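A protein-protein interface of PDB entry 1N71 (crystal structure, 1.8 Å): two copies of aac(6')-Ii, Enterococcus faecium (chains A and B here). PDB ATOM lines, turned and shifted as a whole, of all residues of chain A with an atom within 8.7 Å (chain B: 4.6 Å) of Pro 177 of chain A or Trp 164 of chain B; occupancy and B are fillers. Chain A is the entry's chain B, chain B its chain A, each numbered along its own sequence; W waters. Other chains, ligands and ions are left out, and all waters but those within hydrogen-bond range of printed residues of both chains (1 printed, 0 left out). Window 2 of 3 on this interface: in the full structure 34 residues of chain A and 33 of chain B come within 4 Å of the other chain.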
ATOM      1  N   THR A  69     -25.639  -2.750  23.167  1.00  0.00           N
ATOM      2  CA  THR A  69     -25.921  -1.360  23.513  1.00  0.00           C
ATOM      3  C   THR A  69     -24.654  -0.532  23.744  1.00  0.00           C
ATOM      4  O   THR A  69     -24.618   0.656  23.430  1.00  0.00           O
ATOM      5  CB  THR A  69     -26.805  -1.269  24.783  1.00  0.00           C
ATOM      6  OG1 THR A  69     -26.207  -2.036  25.837  1.00  0.00           O
ATOM      7  CG2 THR A  69     -28.201  -1.812  24.509  1.00  0.00           C
ATOM      8  N   ALA A 100     -25.047   2.543  15.661  1.00  0.00           N
ATOM      9  CA  ALA A 100     -26.461   2.793  15.934  1.00  0.00           C
ATOM     10  C   ALA A 100     -27.353   1.795  15.196  1.00  0.00           C
ATOM     11  O   ALA A 100     -28.310   1.269  15.764  1.00  0.00           O
ATOM     12  CB  ALA A 100     -26.835   4.218  15.527  1.00  0.00           C
ATOM     13  N   GLY A 103     -27.926  -1.365  16.938  1.00  0.00           N
ATOM     14  CA  GLY A 103     -28.503  -1.289  18.271  1.00  0.00           C
ATOM     15  C   GLY A 103     -27.691  -0.576  19.337  1.00  0.00           C
ATOM     16  O   GLY A 103     -28.081  -0.555  20.508  1.00  0.00           O
ATOM     17  N   GLY A 104     -26.571   0.016  18.939  1.00  0.00           N
ATOM     18  CA  GLY A 104     -25.736   0.716  19.893  1.00  0.00           C
ATOM     19  C   GLY A 104     -26.364   1.969  20.480  1.00  0.00           C
ATOM     20  O   GLY A 104     -27.066   2.719  19.798  1.00  0.00           O
ATOM     21  N   ILE A 105     -26.107   2.199  21.760  1.00  0.00           N
ATOM     22  CA  ILE A 105     -26.622   3.372  22.442  1.00  0.00           C
ATOM     23  C   ILE A 105     -25.443   4.262  22.827  1.00  0.00           C
ATOM     24  O   ILE A 105     -25.482   5.484  22.639  1.00  0.00           O
ATOM     25  CB  ILE A 105     -27.396   2.977  23.718  1.00  0.00           C
ATOM     26  CG1 ILE A 105     -28.678   2.231  23.336  1.00  0.00           C
ATOM     27  CG2 ILE A 105     -27.723   4.217  24.545  1.00  0.00           C
ATOM     28  CD1 ILE A 105     -29.496   1.780  24.531  1.00  0.00           C
ATOM     29  N   THR A 106     -24.387   3.631  23.340  1.00  0.00           N
ATOM     30  CA  THR A 106     -23.195   4.340  23.784  1.00  0.00           C
ATOM     31  C   THR A 106     -21.903   3.781  23.198  1.00  0.00           C
ATOM     32  O   THR A 106     -21.744   2.568  23.061  1.00  0.00           O
ATOM     33  CB  THR A 106     -23.069   4.279  25.330  1.00  0.00           C
ATOM     34  OG1 THR A 106     -24.231   4.864  25.929  1.00  0.00           O
ATOM     35  CG2 THR A 106     -21.832   5.030  25.805  1.00  0.00           C
ATOM     36  N   LYS A 173     -19.848   8.698  24.478  1.00  0.00           N
ATOM     37  CA  LYS A 173     -20.868   9.484  23.796  1.00  0.00           C
ATOM     38  C   LYS A 173     -22.090   8.606  23.538  1.00  0.00           C
ATOM     39  O   LYS A 173     -21.959   7.450  23.128  1.00  0.00           O
ATOM     40  CB  LYS A 173     -20.331  10.002  22.458  1.00  0.00           C
ATOM     41  CG  LYS A 173     -21.348  10.773  21.614  1.00  0.00           C
ATOM     42  CD  LYS A 173     -20.724  11.200  20.286  1.00  0.00           C
ATOM     43  CE  LYS A 173     -21.693  12.000  19.430  1.00  0.00           C
ATOM     44  NZ  LYS A 173     -21.054  12.404  18.137  1.00  0.00           N
ATOM     45  N   THR A 174     -23.276   9.140  23.816  1.00  0.00           N
ATOM     46  CA  THR A 174     -24.498   8.400  23.546  1.00  0.00           C
ATOM     47  C   THR A 174     -24.847   8.895  22.152  1.00  0.00           C
ATOM     48  O   THR A 174     -24.969  10.098  21.917  1.00  0.00           O
ATOM     49  CB  THR A 174     -25.582   8.717  24.585  1.00  0.00           C
ATOM     50  OG1 THR A 174     -25.205   8.111  25.832  1.00  0.00           O
ATOM     51  CG2 THR A 174     -26.935   8.160  24.150  1.00  0.00           C
ATOM     52  N   ILE A 175     -24.988   7.953  21.229  1.00  0.00           N
ATOM     53  CA  ILE A 175     -25.196   8.275  19.828  1.00  0.00           C
ATOM     54  C   ILE A 175     -26.597   8.376  19.249  1.00  0.00           C
ATOM     55  O   ILE A 175     -26.746   8.646  18.059  1.00  0.00           O
ATOM     56  CB  ILE A 175     -24.379   7.303  18.971  1.00  0.00           C
ATOM     57  CG1 ILE A 175     -24.851   5.866  19.218  1.00  0.00           C
ATOM     58  CG2 ILE A 175     -22.899   7.434  19.335  1.00  0.00           C
ATOM     59  CD1 ILE A 175     -24.077   4.818  18.430  1.00  0.00           C
ATOM     60  N   ILE A 176     -27.615   8.152  20.069  1.00  0.00           N
ATOM     61  CA  ILE A 176     -28.988   8.267  19.600  1.00  0.00           C
ATOM     62  C   ILE A 176     -29.759   9.134  20.584  1.00  0.00           C
ATOM     63  O   ILE A 176     -29.405   9.218  21.765  1.00  0.00           O
ATOM     64  CB  ILE A 176     -29.692   6.893  19.482  1.00  0.00           C
ATOM     65  CG1 ILE A 176     -29.678   6.175  20.835  1.00  0.00           C
ATOM     66  CG2 ILE A 176     -29.011   6.050  18.419  1.00  0.00           C
ATOM     67  CD1 ILE A 176     -30.560   4.945  20.881  1.00  0.00           C
ATOM     68  N   PRO A 177     -30.815   9.807  20.107  1.00  0.00           N
ATOM     69  CA  PRO A 177     -31.627  10.671  20.967  1.00  0.00           C
ATOM     70  C   PRO A 177     -32.226   9.907  22.143  1.00  0.00           C
ATOM     71  O   PRO A 177     -32.576   8.734  22.021  1.00  0.00           O
ATOM     72  CB  PRO A 177     -32.697  11.192  20.013  1.00  0.00           C
ATOM     73  CG  PRO A 177     -31.975  11.241  18.701  1.00  0.00           C
ATOM     74  CD  PRO A 177     -31.237   9.921  18.699  1.00  0.00           C
ATOM     75  N   ARG A 178     -32.337  10.582  23.280  1.00  0.00           N
ATOM     76  CA  ARG A 178     -32.899   9.981  24.483  1.00  0.00           C
ATOM     77  C   ARG A 178     -34.420   9.941  24.336  1.00  0.00           C
ATOM     78  O   ARG A 178     -35.056  10.973  24.121  1.00  0.00           O
ATOM     79  CB  ARG A 178     -32.507  10.817  25.704  1.00  0.00           C
ATOM     80  CG  ARG A 178     -32.807  10.183  27.049  1.00  0.00           C
ATOM     81  CD  ARG A 178     -32.315  11.088  28.170  1.00  0.00           C
ATOM     82  NE  ARG A 178     -32.574  10.534  29.495  1.00  0.00           N
ATOM     83  CZ  ARG A 178     -31.911   9.513  30.026  1.00  0.00           C
ATOM     84  NH1 ARG A 178     -30.938   8.921  29.350  1.00  0.00           N
ATOM     85  NH2 ARG A 178     -32.225   9.083  31.238  1.00  0.00           N
ATOM     86  N   PRO A 179     -35.021   8.743  24.438  1.00  0.00           N
ATOM     87  CA  PRO A 179     -36.472   8.564  24.316  1.00  0.00           C
ATOM     88  C   PRO A 179     -37.268   9.527  25.192  1.00  0.00           C
ATOM     89  O   PRO A 179     -38.187  10.186  24.659  1.00  0.00           O
ATOM     90  CB  PRO A 179     -36.671   7.107  24.725  1.00  0.00           C
ATOM     91  CG  PRO A 179     -35.414   6.463  24.237  1.00  0.00           C
ATOM     92  CD  PRO A 179     -34.358   7.450  24.679  1.00  0.00           C
ATOM     93  N   ASN B 160     -25.349   4.692  30.201  1.00  0.00           N
ATOM     94  CA  ASN B 160     -26.197   3.872  29.338  1.00  0.00           C
ATOM     95  C   ASN B 160     -25.518   2.650  28.718  1.00  0.00           C
ATOM     96  O   ASN B 160     -25.932   2.181  27.660  1.00  0.00           O
ATOM     97  CB  ASN B 160     -26.757   4.751  28.219  1.00  0.00           C
ATOM     98  CG  ASN B 160     -27.290   6.071  28.735  1.00  0.00           C
ATOM     99  OD1 ASN B 160     -28.154   6.101  29.609  1.00  0.00           O
ATOM    100  ND2 ASN B 160     -26.779   7.173  28.195  1.00  0.00           N
ATOM    101  N   GLY B 163     -27.878  -0.222  28.370  1.00  0.00           N
ATOM    102  CA  GLY B 163     -29.200   0.255  28.005  1.00  0.00           C
ATOM    103  C   GLY B 163     -29.423   1.573  28.719  1.00  0.00           C
ATOM    104  O   GLY B 163     -28.626   1.956  29.572  1.00  0.00           O
ATOM    105  N   TRP B 164     -30.501   2.278  28.397  1.00  0.00           N
ATOM    106  CA  TRP B 164     -30.745   3.560  29.043  1.00  0.00           C
ATOM    107  C   TRP B 164     -30.716   3.502  30.569  1.00  0.00           C
ATOM    108  O   TRP B 164     -31.402   2.696  31.188  1.00  0.00           O
ATOM    109  CB  TRP B 164     -32.075   4.149  28.571  1.00  0.00           C
ATOM    110  CG  TRP B 164     -32.067   4.483  27.111  1.00  0.00           C
ATOM    111  CD1 TRP B 164     -32.689   3.800  26.106  1.00  0.00           C
ATOM    112  CD2 TRP B 164     -31.372   5.570  26.490  1.00  0.00           C
ATOM    113  NE1 TRP B 164     -32.423   4.396  24.893  1.00  0.00           N
ATOM    114  CE2 TRP B 164     -31.616   5.484  25.102  1.00  0.00           C
ATOM    115  CE3 TRP B 164     -30.562   6.608  26.972  1.00  0.00           C
ATOM    116  CZ2 TRP B 164     -31.081   6.399  24.190  1.00  0.00           C
ATOM    117  CZ3 TRP B 164     -30.031   7.519  26.061  1.00  0.00           C
ATOM    118  CH2 TRP B 164     -30.294   7.405  24.687  1.00  0.00           C
ATOM    119  N   ASP B 165     -29.895   4.373  31.150  1.00  0.00           N
ATOM    120  CA  ASP B 165     -29.730   4.506  32.591  1.00  0.00           C
ATOM    121  C   ASP B 165     -29.362   3.238  33.354  1.00  0.00           C
ATOM    122  O   ASP B 165     -29.761   3.056  34.504  1.00  0.00           O
ATOM    123  CB  ASP B 165     -30.979   5.155  33.193  1.00  0.00           C
ATOM    124  CG  ASP B 165     -31.320   6.473  32.521  1.00  0.00           C
ATOM    125  OD1 ASP B 165     -30.385   7.181  32.077  1.00  0.00           O
ATOM    126  OD2 ASP B 165     -32.518   6.807  32.438  1.00  0.00           O
ATOM    127  N   LYS B 166     -28.585   2.377  32.700  1.00  0.00           N
ATOM    128  CA  LYS B 166     -28.089   1.127  33.276  1.00  0.00           C
ATOM    129  C   LYS B 166     -26.597   1.171  32.965  1.00  0.00           C
ATOM    130  O   LYS B 166     -26.095   0.464  32.090  1.00  0.00           O
ATOM    131  CB  LYS B 166     -28.747  -0.071  32.596  1.00  0.00           C
ATOM    132  CG  LYS B 166     -30.250  -0.141  32.840  1.00  0.00           C
ATOM    133  CD  LYS B 166     -30.877  -1.350  32.170  1.00  0.00           C
ATOM    134  CE  LYS B 166     -32.358  -1.437  32.501  1.00  0.00           C
ATOM    135  NZ  LYS B 166     -32.999  -2.627  31.873  1.00  0.00           N
HETATM  136  O   HOH W   1     -27.858   9.865  28.854  1.00  0.00           O
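Of the 13 printed residues of chain A, 8 touch a printed residue of chain B. Hydrophobic or aromatic side chains of chain A that line the printed part of chain B: Ile 105, Ile 176 and Pro 179. Along chain B the printed residues that touch a printed residue of chain A span positions 160 to 165. Among the printed residues, Asp or Glu carboxylates within 4 Å of a Lys or Arg side-chain nitrogen of the other chain: Arg 178 of chain A with Asp 165 of chain B (2.6 Å).
OD1 of Asn 160 of chain B is in hydrogen-bond range of N of Asp 165 of chain B. N of Ile 105 of chain A is in hydrogen-bond range of O of Thr 69 of chain A (2.7 Å). O of Thr 69 of chain A lies within hydrogen-bond range of N of Thr 106 of chain A, 3.0 Å away. N of Ile 175 of chain A sits at hydrogen-bond distance from O of Ile 105 of chain A (2.9 Å). OG1 of Thr 106 of chain A sits at hydrogen-bond distance from OG1 of Thr 174 of chain A (3.4 Å).
Of the printed residues of chain B, Thr 69 of chain A touches Gly 163. Of the printed residues of chain B, Thr 174 of chain A touches Asn 160 and Trp 164. Printed residues of chain B within 4 Å of Ile 176 of chain A: Trp 164 (3.6 Å). Of the printed residues of chain B, Pro 177 of chain A touches Trp 164 (3.5 Å). Trp 164 of chain B touches six residues of chain A. The nearest printed residue of chain B that does not touch Pro 177 of chain A is Asn 160 of chain B (8.6 Å).
No position is printed for both chains. Of the 13 pairs that touch across the chains among the printed residues, none has its exchanged pair printed and touching as well.
Asn 160 of chain B touches Ile 105 of chain A. Gly 163 of chain B touches Ile 105 of chain A. Ile 105 of chain A touches Trp 164 of chain B. Asn 160 of chain B touches Thr 106 of chain A. Trp 164 of chain B touches Thr 174 of chain A. CH2 of Trp 164 of chain B touches O of Ile 176 of chain A, at 3.6 Å. Trp 164 of chain B touches Pro 177 of chain A (CZ2 to O, 3.5 Å). NH1 of Arg 178 of chain A touches OD1 of Asn 160 of chain B, 3.97 Å away. NH1 of Arg 178 of chain A touches CE3 of Trp 164 of chain B (3.3 Å). Pro 179 of chain A touches Trp 164 of chain B.
The side-chain hydroxyl of Thr 174 of chain A is in hydrogen-bond range of the side-chain amide nitrogen of Asn 160 of chain B, 3.0 Å away. The guanidinium group (NH2) of Arg 178 of chain A is in salt-bridge range of the side-chain carboxylate (OD2) of Asp 165 of chain B (2.6 Å).
Water W1 bridges ND2 of Asn 160 of chain B and NH1 of Arg 178 of chain A.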
